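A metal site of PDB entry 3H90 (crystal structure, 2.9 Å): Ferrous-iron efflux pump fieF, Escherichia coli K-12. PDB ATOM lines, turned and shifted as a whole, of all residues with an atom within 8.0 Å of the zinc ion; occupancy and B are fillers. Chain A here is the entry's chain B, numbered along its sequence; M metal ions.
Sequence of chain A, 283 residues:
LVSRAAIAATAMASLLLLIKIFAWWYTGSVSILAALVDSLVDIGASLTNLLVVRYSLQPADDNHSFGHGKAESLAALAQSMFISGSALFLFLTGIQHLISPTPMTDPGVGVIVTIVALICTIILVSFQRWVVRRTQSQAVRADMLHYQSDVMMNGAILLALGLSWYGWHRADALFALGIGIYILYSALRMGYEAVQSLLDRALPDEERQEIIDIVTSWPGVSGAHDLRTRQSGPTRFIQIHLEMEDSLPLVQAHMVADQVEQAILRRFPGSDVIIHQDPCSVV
OD1 of Asp 150 sits close to NE2 of His 146 (3.4 Å).
A ring nitrogen (NE2) of His 146 sits at hydrogen-bond distance from the side-chain carboxylate of Asp 42, at 2.9 Å.
O of Asp 42 lies close to OG of Ser 46 (3.4 Å).
Of the 19 residues printed, 4 come within 4 Å of the zinc ion.
The nearest printed residue that does not touch the zinc ion is Ser 39 (4.5 Å).
The zinc ion is bound by OD2 of Asp 150 (2.0 Å), OD2 of Asp 42 (2.2 Å) and OD1 of Asp 38 (2.3 Å).
Slightly farther from the zinc ion lies a ring nitrogen (NE2) of His 146 (2.6 Å).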
ATOM      1  N   LEU A  17     -27.523 -19.899 -30.765  1.00  0.00           N
ATOM      2  CA  LEU A  17     -26.180 -19.352 -30.873  1.00  0.00           C
ATOM      3  C   LEU A  17     -25.122 -20.389 -30.544  1.00  0.00           C
ATOM      4  O   LEU A  17     -23.958 -20.070 -30.301  1.00  0.00           O
ATOM      5  CB  LEU A  17     -26.030 -18.106 -29.993  1.00  0.00           C
ATOM      6  CG  LEU A  17     -25.494 -16.902 -30.789  1.00  0.00           C
ATOM      7  CD1 LEU A  17     -26.529 -16.407 -31.799  1.00  0.00           C
ATOM      8  CD2 LEU A  17     -25.110 -15.784 -29.883  1.00  0.00           C
ATOM      9  N   LYS A  20     -24.383 -20.580 -34.267  1.00  0.00           N
ATOM     10  CA  LYS A  20     -23.753 -19.352 -34.735  1.00  0.00           C
ATOM     11  C   LYS A  20     -22.290 -19.312 -34.295  1.00  0.00           C
ATOM     12  O   LYS A  20     -21.481 -18.624 -34.908  1.00  0.00           O
ATOM     13  CB  LYS A  20     -24.506 -18.109 -34.278  1.00  0.00           C
ATOM     14  CG  LYS A  20     -24.540 -17.038 -35.341  1.00  0.00           C
ATOM     15  CD  LYS A  20     -24.411 -15.646 -34.761  1.00  0.00           C
ATOM     16  CE  LYS A  20     -22.949 -15.279 -34.497  1.00  0.00           C
ATOM     17  NZ  LYS A  20     -22.776 -13.859 -34.052  1.00  0.00           N
ATOM     18  N   ALA A  35     -15.643 -11.439 -33.251  1.00  0.00           N
ATOM     19  CA  ALA A  35     -17.082 -11.562 -33.006  1.00  0.00           C
ATOM     20  C   ALA A  35     -17.492 -13.028 -32.853  1.00  0.00           C
ATOM     21  O   ALA A  35     -18.691 -13.365 -32.883  1.00  0.00           O
ATOM     22  CB  ALA A  35     -17.882 -10.868 -34.104  1.00  0.00           C
ATOM     23  N   VAL A  37     -16.026 -14.692 -30.210  1.00  0.00           N
ATOM     24  CA  VAL A  37     -16.010 -14.747 -28.753  1.00  0.00           C
ATOM     25  C   VAL A  37     -17.337 -14.191 -28.243  1.00  0.00           C
ATOM     26  O   VAL A  37     -17.876 -14.686 -27.245  1.00  0.00           O
ATOM     27  CB  VAL A  37     -14.833 -13.937 -28.164  1.00  0.00           C
ATOM     28  CG1 VAL A  37     -14.656 -14.238 -26.690  1.00  0.00           C
ATOM     29  CG2 VAL A  37     -13.546 -14.251 -28.908  1.00  0.00           C
ATOM     30  N   ASP A  38     -17.862 -13.194 -28.946  1.00  0.00           N
ATOM     31  CA  ASP A  38     -19.158 -12.585 -28.643  1.00  0.00           C
ATOM     32  C   ASP A  38     -20.247 -13.645 -28.481  1.00  0.00           C
ATOM     33  O   ASP A  38     -21.020 -13.610 -27.518  1.00  0.00           O
ATOM     34  CB  ASP A  38     -19.551 -11.581 -29.737  1.00  0.00           C
ATOM     35  CG  ASP A  38     -20.949 -10.969 -29.524  1.00  0.00           C
ATOM     36  OD1 ASP A  38     -21.460 -10.950 -28.387  1.00  0.00           O
ATOM     37  OD2 ASP A  38     -21.534 -10.490 -30.524  1.00  0.00           O
ATOM     38  N   SER A  39     -20.294 -14.606 -29.399  1.00  0.00           N
ATOM     39  CA  SER A  39     -21.297 -15.649 -29.326  1.00  0.00           C
ATOM     40  C   SER A  39     -20.834 -16.833 -28.460  1.00  0.00           C
ATOM     41  O   SER A  39     -21.664 -17.643 -28.028  1.00  0.00           O
ATOM     42  CB  SER A  39     -21.721 -16.113 -30.728  1.00  0.00           C
ATOM     43  OG  SER A  39     -20.745 -16.946 -31.313  1.00  0.00           O
ATOM     44  N   LEU A  40     -19.536 -16.915 -28.184  1.00  0.00           N
ATOM     45  CA  LEU A  40     -19.048 -17.901 -27.220  1.00  0.00           C
ATOM     46  C   LEU A  40     -19.442 -17.476 -25.812  1.00  0.00           C
ATOM     47  O   LEU A  40     -19.727 -18.315 -24.957  1.00  0.00           O
ATOM     48  CB  LEU A  40     -17.536 -18.086 -27.321  1.00  0.00           C
ATOM     49  CG  LEU A  40     -16.879 -19.033 -26.297  1.00  0.00           C
ATOM     50  CD1 LEU A  40     -17.372 -20.469 -26.433  1.00  0.00           C
ATOM     51  CD2 LEU A  40     -15.369 -18.953 -26.400  1.00  0.00           C
ATOM     52  N   VAL A  41     -19.441 -16.169 -25.558  1.00  0.00           N
ATOM     53  CA  VAL A  41     -19.985 -15.611 -24.330  1.00  0.00           C
ATOM     54  C   VAL A  41     -21.465 -15.990 -24.292  1.00  0.00           C
ATOM     55  O   VAL A  41     -21.913 -16.634 -23.337  1.00  0.00           O
ATOM     56  CB  VAL A  41     -19.802 -14.076 -24.243  1.00  0.00           C
ATOM     57  CG1 VAL A  41     -20.607 -13.482 -23.101  1.00  0.00           C
ATOM     58  CG2 VAL A  41     -18.335 -13.714 -24.091  1.00  0.00           C
ATOM     59  N   ASP A  42     -22.201 -15.620 -25.345  1.00  0.00           N
ATOM     60  CA  ASP A  42     -23.650 -15.848 -25.434  1.00  0.00           C
ATOM     61  C   ASP A  42     -24.087 -17.276 -25.115  1.00  0.00           C
ATOM     62  O   ASP A  42     -25.101 -17.475 -24.464  1.00  0.00           O
ATOM     63  CB  ASP A  42     -24.181 -15.462 -26.815  1.00  0.00           C
ATOM     64  CG  ASP A  42     -24.148 -13.976 -27.054  1.00  0.00           C
ATOM     65  OD1 ASP A  42     -23.503 -13.252 -26.278  1.00  0.00           O
ATOM     66  OD2 ASP A  42     -24.779 -13.511 -28.036  1.00  0.00           O
ATOM     67  N   ILE A  43     -23.326 -18.260 -25.600  1.00  0.00           N
ATOM     68  CA  ILE A  43     -23.637 -19.653 -25.335  1.00  0.00           C
ATOM     69  C   ILE A  43     -23.597 -19.958 -23.833  1.00  0.00           C
ATOM     70  O   ILE A  43     -24.487 -20.622 -23.308  1.00  0.00           O
ATOM     71  CB  ILE A  43     -22.746 -20.640 -26.141  1.00  0.00           C
ATOM     72  CG1 ILE A  43     -23.427 -21.987 -26.278  1.00  0.00           C
ATOM     73  CG2 ILE A  43     -21.376 -20.809 -25.500  1.00  0.00           C
ATOM     74  CD1 ILE A  43     -22.716 -22.922 -27.229  1.00  0.00           C
ATOM     75  N   ALA A  45     -23.497 -17.425 -21.380  1.00  0.00           N
ATOM     76  CA  ALA A  45     -24.414 -16.434 -20.814  1.00  0.00           C
ATOM     77  C   ALA A  45     -25.861 -16.918 -20.818  1.00  0.00           C
ATOM     78  O   ALA A  45     -26.497 -17.029 -19.759  1.00  0.00           O
ATOM     79  CB  ALA A  45     -24.297 -15.105 -21.549  1.00  0.00           C
ATOM     80  N   SER A  46     -26.363 -17.225 -22.013  1.00  0.00           N
ATOM     81  CA  SER A  46     -27.748 -17.620 -22.197  1.00  0.00           C
ATOM     82  C   SER A  46     -28.040 -18.986 -21.571  1.00  0.00           C
ATOM     83  O   SER A  46     -29.170 -19.257 -21.161  1.00  0.00           O
ATOM     84  CB  SER A  46     -28.128 -17.602 -23.661  1.00  0.00           C
ATOM     85  OG  SER A  46     -28.260 -16.265 -24.135  1.00  0.00           O
ATOM     86  N   THR A 121     -30.155 -13.977 -35.768  1.00  0.00           N
ATOM     87  CA  THR A 121     -30.413 -13.188 -34.571  1.00  0.00           C
ATOM     88  C   THR A 121     -31.741 -12.448 -34.690  1.00  0.00           C
ATOM     89  O   THR A 121     -32.518 -12.431 -33.739  1.00  0.00           O
ATOM     90  CB  THR A 121     -29.236 -12.209 -34.278  1.00  0.00           C
ATOM     91  OG1 THR A 121     -27.998 -12.910 -34.415  1.00  0.00           O
ATOM     92  CG2 THR A 121     -29.314 -11.667 -32.873  1.00  0.00           C
ATOM     93  N   HIS A 146     -29.971  -8.029 -25.014  1.00  0.00           N
ATOM     94  CA  HIS A 146     -28.627  -8.252 -25.488  1.00  0.00           C
ATOM     95  C   HIS A 146     -28.612  -8.530 -26.978  1.00  0.00           C
ATOM     96  O   HIS A 146     -27.779  -7.989 -27.705  1.00  0.00           O
ATOM     97  CB  HIS A 146     -27.923  -9.399 -24.781  1.00  0.00           C
ATOM     98  CG  HIS A 146     -26.728  -9.893 -25.527  1.00  0.00           C
ATOM     99  ND1 HIS A 146     -25.649  -9.073 -25.795  1.00  0.00           N
ATOM    100  CD2 HIS A 146     -26.464 -11.067 -26.144  1.00  0.00           C
ATOM    101  CE1 HIS A 146     -24.755  -9.744 -26.498  1.00  0.00           C
ATOM    102  NE2 HIS A 146     -25.238 -10.957 -26.730  1.00  0.00           N
ATOM    103  N   TYR A 147     -29.534  -9.387 -27.436  1.00  0.00           N
ATOM    104  CA  TYR A 147     -29.570  -9.814 -28.829  1.00  0.00           C
ATOM    105  C   TYR A 147     -30.080  -8.716 -29.747  1.00  0.00           C
ATOM    106  O   TYR A 147     -29.690  -8.656 -30.899  1.00  0.00           O
ATOM    107  CB  TYR A 147     -30.384 -11.088 -28.984  1.00  0.00           C
ATOM    108  CG  TYR A 147     -29.719 -12.274 -28.336  1.00  0.00           C
ATOM    109  CD1 TYR A 147     -30.269 -12.872 -27.197  1.00  0.00           C
ATOM    110  CD2 TYR A 147     -28.535 -12.792 -28.851  1.00  0.00           C
ATOM    111  CE1 TYR A 147     -29.651 -13.968 -26.593  1.00  0.00           C
ATOM    112  CE2 TYR A 147     -27.907 -13.880 -28.268  1.00  0.00           C
ATOM    113  CZ  TYR A 147     -28.448 -14.457 -27.146  1.00  0.00           C
ATOM    114  OH  TYR A 147     -27.793 -15.533 -26.594  1.00  0.00           O
ATOM    115  N   SER A 149     -29.068  -5.849 -29.397  1.00  0.00           N
ATOM    116  CA  SER A 149     -27.797  -5.180 -29.617  1.00  0.00           C
ATOM    117  C   SER A 149     -27.001  -5.900 -30.682  1.00  0.00           C
ATOM    118  O   SER A 149     -26.474  -5.273 -31.589  1.00  0.00           O
ATOM    119  CB  SER A 149     -27.003  -5.097 -28.317  1.00  0.00           C
ATOM    120  OG  SER A 149     -25.635  -4.830 -28.587  1.00  0.00           O
ATOM    121  N   ASP A 150     -26.912  -7.231 -30.577  1.00  0.00           N
ATOM    122  CA  ASP A 150     -26.226  -8.030 -31.596  1.00  0.00           C
ATOM    123  C   ASP A 150     -26.845  -7.788 -32.978  1.00  0.00           C
ATOM    124  O   ASP A 150     -26.134  -7.763 -33.985  1.00  0.00           O
ATOM    125  CB  ASP A 150     -26.281  -9.523 -31.256  1.00  0.00           C
ATOM    126  CG  ASP A 150     -25.379  -9.903 -30.088  1.00  0.00           C
ATOM    127  OD1 ASP A 150     -24.784  -9.010 -29.449  1.00  0.00           O
ATOM    128  OD2 ASP A 150     -25.266 -11.107 -29.794  1.00  0.00           O
ATOM    129  N   VAL A 151     -28.158  -7.608 -33.004  1.00  0.00           N
ATOM    130  CA  VAL A 151     -28.919  -7.345 -34.221  1.00  0.00           C
ATOM    131  C   VAL A 151     -28.521  -6.024 -34.845  1.00  0.00           C
ATOM    132  O   VAL A 151     -28.700  -5.830 -36.045  1.00  0.00           O
ATOM    133  CB  VAL A 151     -30.453  -7.422 -33.958  1.00  0.00           C
ATOM    134  CG1 VAL A 151     -31.234  -6.399 -34.781  1.00  0.00           C
ATOM    135  CG2 VAL A 151     -30.976  -8.812 -34.244  1.00  0.00           C
ATOM    136  N   MET A 153     -25.887  -4.916 -36.055  1.00  0.00           N
ATOM    137  CA  MET A 153     -24.633  -5.335 -36.636  1.00  0.00           C
ATOM    138  C   MET A 153     -24.518  -4.659 -37.977  1.00  0.00           C
ATOM    139  O   MET A 153     -25.495  -4.600 -38.737  1.00  0.00           O
ATOM    140  CB  MET A 153     -24.657  -6.846 -36.848  1.00  0.00           C
ATOM    141  CG  MET A 153     -23.356  -7.510 -36.587  1.00  0.00           C
ATOM    142  SD  MET A 153     -23.580  -9.284 -36.617  1.00  0.00           S
ATOM    143  CE  MET A 153     -22.126  -9.866 -35.752  1.00  0.00           C
HETATM  144 ZN    ZN M   1     -23.644 -11.699 -28.691  1.00  0.00          ZN
